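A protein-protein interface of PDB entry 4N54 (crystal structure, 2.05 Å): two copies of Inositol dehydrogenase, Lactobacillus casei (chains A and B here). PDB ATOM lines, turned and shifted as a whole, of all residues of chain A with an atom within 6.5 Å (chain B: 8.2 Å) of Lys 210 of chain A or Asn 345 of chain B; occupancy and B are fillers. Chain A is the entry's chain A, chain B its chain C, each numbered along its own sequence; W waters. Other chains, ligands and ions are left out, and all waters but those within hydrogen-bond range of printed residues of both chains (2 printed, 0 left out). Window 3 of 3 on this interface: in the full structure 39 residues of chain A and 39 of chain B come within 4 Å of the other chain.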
ATOM      1  N   ILE A 208      10.365 -23.287  36.425  1.00  0.00           N
ATOM      2  CA  ILE A 208      10.561 -22.896  35.049  1.00  0.00           C
ATOM      3  C   ILE A 208       9.230 -22.574  34.393  1.00  0.00           C
ATOM      4  O   ILE A 208       8.297 -23.336  34.492  1.00  0.00           O
ATOM      5  CB  ILE A 208      11.275 -23.985  34.265  1.00  0.00           C
ATOM      6  CG1 ILE A 208      12.680 -24.198  34.835  1.00  0.00           C
ATOM      7  CG2 ILE A 208      11.362 -23.602  32.829  1.00  0.00           C
ATOM      8  CD1 ILE A 208      13.230 -25.525  34.622  1.00  0.00           C
ATOM      9  N   ASP A 209       9.164 -21.428  33.741  1.00  0.00           N
ATOM     10  CA  ASP A 209       7.957 -20.998  33.069  1.00  0.00           C
ATOM     11  C   ASP A 209       7.897 -21.434  31.618  1.00  0.00           C
ATOM     12  O   ASP A 209       7.014 -22.185  31.252  1.00  0.00           O
ATOM     13  CB  ASP A 209       7.776 -19.493  33.156  1.00  0.00           C
ATOM     14  CG  ASP A 209       6.588 -19.017  32.367  1.00  0.00           C
ATOM     15  OD1 ASP A 209       5.495 -19.549  32.570  1.00  0.00           O
ATOM     16  OD2 ASP A 209       6.745 -18.137  31.517  1.00  0.00           O
ATOM     17  N   LYS A 210       8.799 -20.936  30.790  1.00  0.00           N
ATOM     18  CA  LYS A 210       8.823 -21.351  29.399  1.00  0.00           C
ATOM     19  C   LYS A 210      10.212 -21.609  28.837  1.00  0.00           C
ATOM     20  O   LYS A 210      11.193 -21.044  29.294  1.00  0.00           O
ATOM     21  CB  LYS A 210       8.040 -20.399  28.507  1.00  0.00           C
ATOM     22  CG  LYS A 210       8.541 -18.999  28.410  1.00  0.00           C
ATOM     23  CD  LYS A 210       7.459 -18.110  27.812  1.00  0.00           C
ATOM     24  CE  LYS A 210       8.023 -17.014  26.971  1.00  0.00           C
ATOM     25  NZ  LYS A 210       6.975 -16.309  26.196  1.00  0.00           N
ATOM     26  N   VAL A 211      10.267 -22.485  27.844  1.00  0.00           N
ATOM     27  CA  VAL A 211      11.520 -22.946  27.268  1.00  0.00           C
ATOM     28  C   VAL A 211      11.489 -22.951  25.743  1.00  0.00           C
ATOM     29  O   VAL A 211      10.430 -23.012  25.139  1.00  0.00           O
ATOM     30  CB  VAL A 211      11.906 -24.361  27.779  1.00  0.00           C
ATOM     31  CG1 VAL A 211      11.870 -24.424  29.271  1.00  0.00           C
ATOM     32  CG2 VAL A 211      10.993 -25.414  27.216  1.00  0.00           C
ATOM     33  N   TRP A 212      12.663 -22.837  25.142  1.00  0.00           N
ATOM     34  CA  TRP A 212      12.875 -23.181  23.739  1.00  0.00           C
ATOM     35  C   TRP A 212      14.134 -24.042  23.668  1.00  0.00           C
ATOM     36  O   TRP A 212      15.122 -23.726  24.298  1.00  0.00           O
ATOM     37  CB  TRP A 212      13.035 -21.944  22.869  1.00  0.00           C
ATOM     38  CG  TRP A 212      13.256 -22.238  21.418  1.00  0.00           C
ATOM     39  CD1 TRP A 212      12.734 -23.273  20.708  1.00  0.00           C
ATOM     40  CD2 TRP A 212      14.064 -21.503  20.503  1.00  0.00           C
ATOM     41  NE1 TRP A 212      13.163 -23.231  19.419  1.00  0.00           N
ATOM     42  CE2 TRP A 212      13.980 -22.150  19.265  1.00  0.00           C
ATOM     43  CE3 TRP A 212      14.850 -20.369  20.610  1.00  0.00           C
ATOM     44  CZ2 TRP A 212      14.649 -21.696  18.153  1.00  0.00           C
ATOM     45  CZ3 TRP A 212      15.509 -19.924  19.509  1.00  0.00           C
ATOM     46  CH2 TRP A 212      15.406 -20.580  18.296  1.00  0.00           C
ATOM     47  N   LEU A 235      17.164 -22.329  25.882  1.00  0.00           N
ATOM     48  CA  LEU A 235      16.949 -21.127  26.666  1.00  0.00           C
ATOM     49  C   LEU A 235      15.678 -21.298  27.489  1.00  0.00           C
ATOM     50  O   LEU A 235      14.661 -21.726  26.974  1.00  0.00           O
ATOM     51  CB  LEU A 235      16.820 -19.930  25.747  1.00  0.00           C
ATOM     52  CG  LEU A 235      16.562 -18.561  26.347  1.00  0.00           C
ATOM     53  CD1 LEU A 235      17.631 -18.202  27.316  1.00  0.00           C
ATOM     54  CD2 LEU A 235      16.521 -17.547  25.273  1.00  0.00           C
ATOM     55  N   MET A 236      15.761 -21.001  28.779  1.00  0.00           N
ATOM     56  CA  MET A 236      14.611 -21.083  29.662  1.00  0.00           C
ATOM     57  C   MET A 236      14.400 -19.781  30.429  1.00  0.00           C
ATOM     58  O   MET A 236      15.348 -19.095  30.763  1.00  0.00           O
ATOM     59  CB  MET A 236      14.743 -22.238  30.641  1.00  0.00           C
ATOM     60  CG  MET A 236      15.190 -23.530  30.029  1.00  0.00           C
ATOM     61  SD  MET A 236      14.835 -24.981  30.991  1.00  0.00           S
ATOM     62  CE  MET A 236      15.842 -24.683  32.391  1.00  0.00           C
ATOM     63  N   GLN A 237      13.145 -19.446  30.680  1.00  0.00           N
ATOM     64  CA  GLN A 237      12.784 -18.295  31.491  1.00  0.00           C
ATOM     65  C   GLN A 237      12.000 -18.813  32.655  1.00  0.00           C
ATOM     66  O   GLN A 237      11.044 -19.539  32.479  1.00  0.00           O
ATOM     67  CB  GLN A 237      11.931 -17.311  30.710  1.00  0.00           C
ATOM     68  CG  GLN A 237      11.579 -16.054  31.441  1.00  0.00           C
ATOM     69  CD  GLN A 237      10.956 -15.028  30.553  1.00  0.00           C
ATOM     70  OE1 GLN A 237       9.907 -15.252  29.976  1.00  0.00           O
ATOM     71  NE2 GLN A 237      11.598 -13.896  30.431  1.00  0.00           N
ATOM     72  N   LEU A 238      12.428 -18.470  33.854  1.00  0.00           N
ATOM     73  CA  LEU A 238      11.741 -18.928  35.037  1.00  0.00           C
ATOM     74  C   LEU A 238      10.594 -17.980  35.408  1.00  0.00           C
ATOM     75  O   LEU A 238      10.426 -16.935  34.819  1.00  0.00           O
ATOM     76  CB  LEU A 238      12.709 -19.088  36.200  1.00  0.00           C
ATOM     77  CG  LEU A 238      13.662 -20.282  36.254  1.00  0.00           C
ATOM     78  CD1 LEU A 238      14.668 -20.280  35.138  1.00  0.00           C
ATOM     79  CD2 LEU A 238      14.356 -20.288  37.593  1.00  0.00           C
ATOM     80  N   GLU A 239       9.828 -18.359  36.408  1.00  0.00           N
ATOM     81  CA  GLU A 239       8.647 -17.611  36.796  1.00  0.00           C
ATOM     82  C   GLU A 239       8.945 -16.195  37.297  1.00  0.00           C
ATOM     83  O   GLU A 239       8.123 -15.312  37.165  1.00  0.00           O
ATOM     84  CB  GLU A 239       7.845 -18.402  37.819  1.00  0.00           C
ATOM     85  CG  GLU A 239       8.578 -18.688  39.100  1.00  0.00           C
ATOM     86  CD  GLU A 239       7.802 -19.569  40.048  1.00  0.00           C
ATOM     87  OE1 GLU A 239       6.559 -19.628  39.934  1.00  0.00           O
ATOM     88  OE2 GLU A 239       8.436 -20.220  40.897  1.00  0.00           O
ATOM     89  N   LYS A 241      11.453 -14.399  36.098  1.00  0.00           N
ATOM     90  CA  LYS A 241      12.262 -13.842  35.021  1.00  0.00           C
ATOM     91  C   LYS A 241      13.772 -14.117  35.113  1.00  0.00           C
ATOM     92  O   LYS A 241      14.533 -13.607  34.329  1.00  0.00           O
ATOM     93  CB  LYS A 241      11.993 -12.351  34.843  1.00  0.00           C
ATOM     94  CG  LYS A 241      10.527 -11.995  34.688  1.00  0.00           C
ATOM     95  CD  LYS A 241       9.888 -12.757  33.549  1.00  0.00           C
ATOM     96  CE  LYS A 241       8.367 -12.606  33.570  1.00  0.00           C
ATOM     97  NZ  LYS A 241       7.667 -13.905  33.410  1.00  0.00           N
ATOM     98  N   ILE A 347       8.693 -22.194  21.142  1.00  0.00           N
ATOM     99  CA  ILE A 347       8.601 -22.016  22.576  1.00  0.00           C
ATOM    100  C   ILE A 347       7.507 -22.882  23.197  1.00  0.00           C
ATOM    101  O   ILE A 347       6.442 -23.024  22.634  1.00  0.00           O
ATOM    102  CB  ILE A 347       8.406 -20.520  22.902  1.00  0.00           C
ATOM    103  CG1 ILE A 347       9.714 -19.767  22.673  1.00  0.00           C
ATOM    104  CG2 ILE A 347       7.906 -20.336  24.302  1.00  0.00           C
ATOM    105  CD1 ILE A 347       9.596 -18.317  22.528  1.00  0.00           C
ATOM    106  N   VAL A 348       7.791 -23.483  24.342  1.00  0.00           N
ATOM    107  CA  VAL A 348       6.796 -24.236  25.094  1.00  0.00           C
ATOM    108  C   VAL A 348       6.650 -23.749  26.555  1.00  0.00           C
ATOM    109  O   VAL A 348       7.614 -23.349  27.178  1.00  0.00           O
ATOM    110  CB  VAL A 348       7.104 -25.737  25.045  1.00  0.00           C
ATOM    111  CG1 VAL A 348       6.192 -26.532  25.949  1.00  0.00           C
ATOM    112  CG2 VAL A 348       7.003 -26.229  23.633  1.00  0.00           C
ATOM    113  N   GLN A 349       5.424 -23.758  27.065  1.00  0.00           N
ATOM    114  CA  GLN A 349       5.133 -23.436  28.454  1.00  0.00           C
ATOM    115  C   GLN A 349       5.163 -24.681  29.295  1.00  0.00           C
ATOM    116  O   GLN A 349       4.598 -25.688  28.915  1.00  0.00           O
ATOM    117  CB  GLN A 349       3.746 -22.832  28.578  1.00  0.00           C
ATOM    118  CG  GLN A 349       3.538 -21.588  27.800  1.00  0.00           C
ATOM    119  CD  GLN A 349       3.631 -20.358  28.655  1.00  0.00           C
ATOM    120  OE1 GLN A 349       3.697 -20.440  29.881  1.00  0.00           O
ATOM    121  NE2 GLN A 349       3.636 -19.199  28.016  1.00  0.00           N
ATOM    122  N   VAL A 350       5.803 -24.614  30.451  1.00  0.00           N
ATOM    123  CA  VAL A 350       5.872 -25.772  31.314  1.00  0.00           C
ATOM    124  C   VAL A 350       4.520 -26.109  31.940  1.00  0.00           C
ATOM    125  O   VAL A 350       4.202 -27.272  32.131  1.00  0.00           O
ATOM    126  CB  VAL A 350       6.938 -25.614  32.401  1.00  0.00           C
ATOM    127  CG1 VAL A 350       7.121 -26.901  33.162  1.00  0.00           C
ATOM    128  CG2 VAL A 350       8.240 -25.177  31.789  1.00  0.00           C
ATOM    129  N   VAL B 211      15.889 -16.365  16.206  1.00  0.00           N
ATOM    130  CA  VAL B 211      16.419 -16.034  17.516  1.00  0.00           C
ATOM    131  C   VAL B 211      15.318 -15.863  18.560  1.00  0.00           C
ATOM    132  O   VAL B 211      14.192 -15.507  18.234  1.00  0.00           O
ATOM    133  CB  VAL B 211      17.238 -14.738  17.467  1.00  0.00           C
ATOM    134  CG1 VAL B 211      18.226 -14.761  16.341  1.00  0.00           C
ATOM    135  CG2 VAL B 211      16.336 -13.529  17.335  1.00  0.00           C
ATOM    136  N   TRP B 212      15.644 -16.150  19.814  1.00  0.00           N
ATOM    137  CA  TRP B 212      14.797 -15.785  20.935  1.00  0.00           C
ATOM    138  C   TRP B 212      15.657 -15.162  22.023  1.00  0.00           C
ATOM    139  O   TRP B 212      16.735 -15.651  22.299  1.00  0.00           O
ATOM    140  CB  TRP B 212      14.063 -16.981  21.499  1.00  0.00           C
ATOM    141  CG  TRP B 212      13.192 -16.643  22.655  1.00  0.00           C
ATOM    142  CD1 TRP B 212      12.452 -15.522  22.809  1.00  0.00           C
ATOM    143  CD2 TRP B 212      12.990 -17.415  23.831  1.00  0.00           C
ATOM    144  NE1 TRP B 212      11.799 -15.549  23.996  1.00  0.00           N
ATOM    145  CE2 TRP B 212      12.118 -16.702  24.652  1.00  0.00           C
ATOM    146  CE3 TRP B 212      13.470 -18.642  24.276  1.00  0.00           C
ATOM    147  CZ2 TRP B 212      11.704 -17.173  25.869  1.00  0.00           C
ATOM    148  CZ3 TRP B 212      13.059 -19.102  25.474  1.00  0.00           C
ATOM    149  CH2 TRP B 212      12.181 -18.378  26.262  1.00  0.00           C
ATOM    150  N   ALA B 213      15.169 -14.083  22.631  1.00  0.00           N
ATOM    151  CA  ALA B 213      15.899 -13.362  23.662  1.00  0.00           C
ATOM    152  C   ALA B 213      15.048 -13.068  24.879  1.00  0.00           C
ATOM    153  O   ALA B 213      13.869 -12.759  24.772  1.00  0.00           O
ATOM    154  CB  ALA B 213      16.438 -12.097  23.117  1.00  0.00           C
ATOM    155  N   ILE B 214      15.668 -13.174  26.042  1.00  0.00           N
ATOM    156  CA  ILE B 214      15.059 -12.761  27.291  1.00  0.00           C
ATOM    157  C   ILE B 214      15.981 -11.795  28.039  1.00  0.00           C
ATOM    158  O   ILE B 214      17.133 -11.641  27.692  1.00  0.00           O
ATOM    159  CB  ILE B 214      14.640 -13.952  28.143  1.00  0.00           C
ATOM    160  CG1 ILE B 214      15.811 -14.906  28.389  1.00  0.00           C
ATOM    161  CG2 ILE B 214      13.511 -14.685  27.469  1.00  0.00           C
ATOM    162  CD1 ILE B 214      15.471 -16.047  29.221  1.00  0.00           C
ATOM    163  N   GLY B 215      15.457 -11.122  29.044  1.00  0.00           N
ATOM    164  CA  GLY B 215      16.204 -10.085  29.721  1.00  0.00           C
ATOM    165  C   GLY B 215      15.733  -9.906  31.139  1.00  0.00           C
ATOM    166  O   GLY B 215      14.635 -10.318  31.488  1.00  0.00           O
ATOM    167  N   LEU B 338      17.027  -9.667  17.677  1.00  0.00           N
ATOM    168  CA  LEU B 338      17.170 -10.012  19.075  1.00  0.00           C
ATOM    169  C   LEU B 338      16.340  -9.061  19.928  1.00  0.00           C
ATOM    170  O   LEU B 338      15.654  -9.461  20.843  1.00  0.00           O
ATOM    171  CB  LEU B 338      18.648  -9.947  19.450  1.00  0.00           C
ATOM    172  CG  LEU B 338      19.510 -11.093  18.911  1.00  0.00           C
ATOM    173  CD1 LEU B 338      20.964 -10.778  18.962  1.00  0.00           C
ATOM    174  CD2 LEU B 338      19.225 -12.349  19.670  1.00  0.00           C
ATOM    175  N   GLN B 339      16.423  -7.791  19.580  1.00  0.00           N
ATOM    176  CA  GLN B 339      15.711  -6.738  20.257  1.00  0.00           C
ATOM    177  C   GLN B 339      14.216  -6.956  20.118  1.00  0.00           C
ATOM    178  O   GLN B 339      13.493  -6.921  21.092  1.00  0.00           O
ATOM    179  CB  GLN B 339      16.130  -5.400  19.689  1.00  0.00           C
ATOM    180  CG  GLN B 339      16.117  -4.270  20.698  1.00  0.00           C
ATOM    181  CD  GLN B 339      17.065  -4.488  21.859  1.00  0.00           C
ATOM    182  OE1 GLN B 339      18.243  -4.767  21.668  1.00  0.00           O
ATOM    183  NE2 GLN B 339      16.552  -4.367  23.063  1.00  0.00           N
ATOM    184  N   GLU B 340      13.776  -7.239  18.900  1.00  0.00           N
ATOM    185  CA  GLU B 340      12.377  -7.535  18.638  1.00  0.00           C
ATOM    186  C   GLU B 340      11.907  -8.773  19.363  1.00  0.00           C
ATOM    187  O   GLU B 340      10.809  -8.805  19.884  1.00  0.00           O
ATOM    188  CB  GLU B 340      12.112  -7.666  17.139  1.00  0.00           C
ATOM    189  CG  GLU B 340      10.671  -7.989  16.803  1.00  0.00           C
ATOM    190  CD  GLU B 340      10.395  -8.030  15.324  1.00  0.00           C
ATOM    191  OE1 GLU B 340      11.213  -7.504  14.558  1.00  0.00           O
ATOM    192  OE2 GLU B 340       9.358  -8.581  14.927  1.00  0.00           O
ATOM    193  N   ALA B 341      12.742  -9.795  19.408  1.00  0.00           N
ATOM    194  CA  ALA B 341      12.360 -11.016  20.082  1.00  0.00           C
ATOM    195  C   ALA B 341      12.255 -10.790  21.583  1.00  0.00           C
ATOM    196  O   ALA B 341      11.457 -11.405  22.263  1.00  0.00           O
ATOM    197  CB  ALA B 341      13.329 -12.113  19.775  1.00  0.00           C
ATOM    198  N   PHE B 342      13.086  -9.896  22.089  1.00  0.00           N
ATOM    199  CA  PHE B 342      13.021  -9.539  23.482  1.00  0.00           C
ATOM    200  C   PHE B 342      11.704  -8.825  23.793  1.00  0.00           C
ATOM    201  O   PHE B 342      11.047  -9.134  24.762  1.00  0.00           O
ATOM    202  CB  PHE B 342      14.183  -8.643  23.874  1.00  0.00           C
ATOM    203  CG  PHE B 342      13.988  -7.993  25.190  1.00  0.00           C
ATOM    204  CD1 PHE B 342      13.962  -8.740  26.334  1.00  0.00           C
ATOM    205  CD2 PHE B 342      13.782  -6.634  25.283  1.00  0.00           C
ATOM    206  CE1 PHE B 342      13.768  -8.148  27.544  1.00  0.00           C
ATOM    207  CE2 PHE B 342      13.578  -6.042  26.497  1.00  0.00           C
ATOM    208  CZ  PHE B 342      13.570  -6.792  27.620  1.00  0.00           C
ATOM    209  N   GLU B 343      11.349  -7.862  22.959  1.00  0.00           N
ATOM    210  CA  GLU B 343      10.162  -7.067  23.190  1.00  0.00           C
ATOM    211  C   GLU B 343       8.915  -7.924  23.121  1.00  0.00           C
ATOM    212  O   GLU B 343       8.004  -7.760  23.903  1.00  0.00           O
ATOM    213  CB  GLU B 343      10.114  -5.891  22.226  1.00  0.00           C
ATOM    214  CG  GLU B 343      11.186  -4.871  22.509  1.00  0.00           C
ATOM    215  CD  GLU B 343      11.311  -3.825  21.444  1.00  0.00           C
ATOM    216  OE1 GLU B 343      10.424  -3.747  20.588  1.00  0.00           O
ATOM    217  OE2 GLU B 343      12.289  -3.060  21.461  1.00  0.00           O
ATOM    218  N   LYS B 344       8.915  -8.894  22.225  1.00  0.00           N
ATOM    219  CA  LYS B 344       7.776  -9.765  22.061  1.00  0.00           C
ATOM    220  C   LYS B 344       7.818 -10.964  22.966  1.00  0.00           C
ATOM    221  O   LYS B 344       6.814 -11.618  23.166  1.00  0.00           O
ATOM    222  CB  LYS B 344       7.658 -10.193  20.606  1.00  0.00           C
ATOM    223  CG  LYS B 344       7.602  -9.002  19.682  1.00  0.00           C
ATOM    224  CD  LYS B 344       6.811  -9.242  18.420  1.00  0.00           C
ATOM    225  CE  LYS B 344       7.644  -9.908  17.365  1.00  0.00           C
ATOM    226  NZ  LYS B 344       7.450  -9.250  16.061  1.00  0.00           N
ATOM    227  N   ASN B 345       8.981 -11.217  23.548  1.00  0.00           N
ATOM    228  CA  ASN B 345       9.239 -12.461  24.239  1.00  0.00           C
ATOM    229  C   ASN B 345       8.762 -13.651  23.414  1.00  0.00           C
ATOM    230  O   ASN B 345       7.931 -14.425  23.847  1.00  0.00           O
ATOM    231  CB  ASN B 345       8.653 -12.474  25.645  1.00  0.00           C
ATOM    232  CG  ASN B 345       9.220 -13.580  26.491  1.00  0.00           C
ATOM    233  OD1 ASN B 345      10.084 -14.309  26.056  1.00  0.00           O
ATOM    234  ND2 ASN B 345       8.732 -13.709  27.698  1.00  0.00           N
ATOM    235  N   ASP B 346       9.314 -13.771  22.215  1.00  0.00           N
ATOM    236  CA  ASP B 346       8.927 -14.805  21.281  1.00  0.00           C
ATOM    237  C   ASP B 346      10.032 -14.972  20.258  1.00  0.00           C
ATOM    238  O   ASP B 346      10.903 -14.131  20.146  1.00  0.00           O
ATOM    239  CB  ASP B 346       7.635 -14.402  20.580  1.00  0.00           C
ATOM    240  CG  ASP B 346       6.911 -15.580  19.927  1.00  0.00           C
ATOM    241  OD1 ASP B 346       6.987 -16.711  20.424  1.00  0.00           O
ATOM    242  OD2 ASP B 346       6.247 -15.346  18.912  1.00  0.00           O
ATOM    243  N   ILE B 347       9.984 -16.067  19.512  1.00  0.00           N
ATOM    244  CA  ILE B 347      10.952 -16.320  18.458  1.00  0.00           C
ATOM    245  C   ILE B 347      10.730 -15.419  17.259  1.00  0.00           C
ATOM    246  O   ILE B 347       9.603 -15.160  16.878  1.00  0.00           O
ATOM    247  CB  ILE B 347      10.941 -17.794  18.043  1.00  0.00           C
ATOM    248  CG1 ILE B 347      11.357 -18.647  19.222  1.00  0.00           C
ATOM    249  CG2 ILE B 347      11.869 -18.021  16.897  1.00  0.00           C
ATOM    250  CD1 ILE B 347      10.982 -20.033  19.140  1.00  0.00           C
ATOM    251  N   VAL B 348      11.817 -14.925  16.690  1.00  0.00           N
ATOM    252  CA  VAL B 348      11.769 -14.032  15.556  1.00  0.00           C
ATOM    253  C   VAL B 348      12.674 -14.527  14.428  1.00  0.00           C
ATOM    254  O   VAL B 348      13.815 -14.911  14.672  1.00  0.00           O
ATOM    255  CB  VAL B 348      12.195 -12.611  15.971  1.00  0.00           C
ATOM    256  CG1 VAL B 348      12.431 -11.747  14.782  1.00  0.00           C
ATOM    257  CG2 VAL B 348      11.164 -11.992  16.850  1.00  0.00           C
HETATM  258  O   HOH W   1      14.037 -12.977  31.550  1.00  0.00           O
HETATM  259  O   HOH W   2      12.226 -10.965  28.915  1.00  0.00           O
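Trp 212 of chain A touches its own counterpart, Trp 212 of chain B. Trp 212 of chain A touches Ile 347 of chain B, and with the chains exchanged Ile 347 of chain A touches Trp 212 of chain B. Ile 347 of chain A touches its own counterpart, Ile 347 of chain B. Positions printed for both chains: 211, 212, 347 and 348. Of the 12 pairs that touch across the chains among the printed residues, 4 have their exchanged pair printed and touching as well.
Lys 210 of chain A touches Trp 212 of chain B. CE3 of Trp 212 of chain A touches CB of Trp 212 of chain B, at 3.6 Å. CD1 of Ile 347 of chain B touches CE2 of Trp 212 of chain A (3.7 Å). Leu 235 of chain A touches Trp 212 of chain B (CD2 to CE3, 3.4 Å). CD1 of Ile 214 of chain B touches CD1 of Leu 235 of chain A, at 3.6 Å. Met 236 of chain A touches Ile 214 of chain B (O to CD1, 3.4 Å). Gln 237 of chain A touches Ile 214 of chain B. CD1 of Ile 347 of chain A touches CE2 of Trp 212 of chain B, at 3.7 Å. OD1 of Asp 346 of chain B touches CD1 of Ile 347 of chain A, 3.7 Å away. Ile 347 of chain B touches Ile 347 of chain A (CD1 to N, 3.7 Å).
NZ of Lys 210 of chain A is in hydrogen-bond range of O of Asn 345 of chain B, at 3.2 Å. ND2 of Asn 345 of chain B is in hydrogen-bond range of OE1 of Gln 237 of chain A (3.0 Å).
Of the 15 printed residues of chain A, 6 touch a printed residue of chain B. Printed residues of chain A that touch a printed residue of chain B: Lys 210, Trp 212, Leu 235, Met 236, Gln 237 and Ile 347. Hydrophobic or aromatic side chains of chain A that line the printed part of chain B: Trp 212, Leu 235 and Ile 347. Among the printed residues, no Asp or Glu carboxylate lies within 4 Å of a Lys or Arg side-chain nitrogen of the other chain.
O of Lys 210 of chain A lies within hydrogen-bond range of N of Gln 237 of chain A. The backbone carbonyl oxygen of Leu 235 of chain A lies within hydrogen-bond range of the backbone NH of Trp 212 of chain A, at 2.9 Å. N of Asp 346 of chain B lies within hydrogen-bond range of O of Ala 341 of chain B (3.2 Å). O of Gln 237 of chain A sits at hydrogen-bond distance from N of Asp 209 of chain A (2.9 Å). The indole nitrogen (NE1) of Trp 212 of chain B lies within hydrogen-bond range of the side-chain amide oxygen (OD1) of Asn 345 of chain B, 3.0 Å away.
Lys 210 of chain A touches two residues of chain B. Asn 345 of chain B touches just these residues of chain A: Lys 210 (3.2 Å) and Gln 237 (3.0 Å). Of the printed residues of chain B, Gln 237 of chain A touches Ile 214 (3.6 Å) and Asn 345 (3.0 Å). Printed residues of chain B within 4 Å of Leu 235 of chain A: Trp 212 (3.4 Å) and Ile 214 (3.6 Å). Of the printed residues of chain A, Ile 214 of chain B touches Leu 235, Met 236 and Gln 237. Ala 213 of chain B touches none of the printed residues of chain A. The nearest residue of chain A that does not touch Asn 345 of chain B is Ile 347 of chain A (4.4 Å). The nearest printed residue of chain B that does not touch Leu 235 of chain A is Ala 213 of chain B (4.5 Å).
Water W1 lies within hydrogen-bond range of O of Gly 215 of chain B (2.7 Å), NE2 of Gln 237 of chain A (2.8 Å) and O of Lys 241 of chain A (2.9 Å). Water W2 bridges the backbone NH (N) of Gly 215 of chain B (3.2 Å) and the side-chain amide nitrogen (NE2) of Gln 237 of chain A (3.4 Å).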
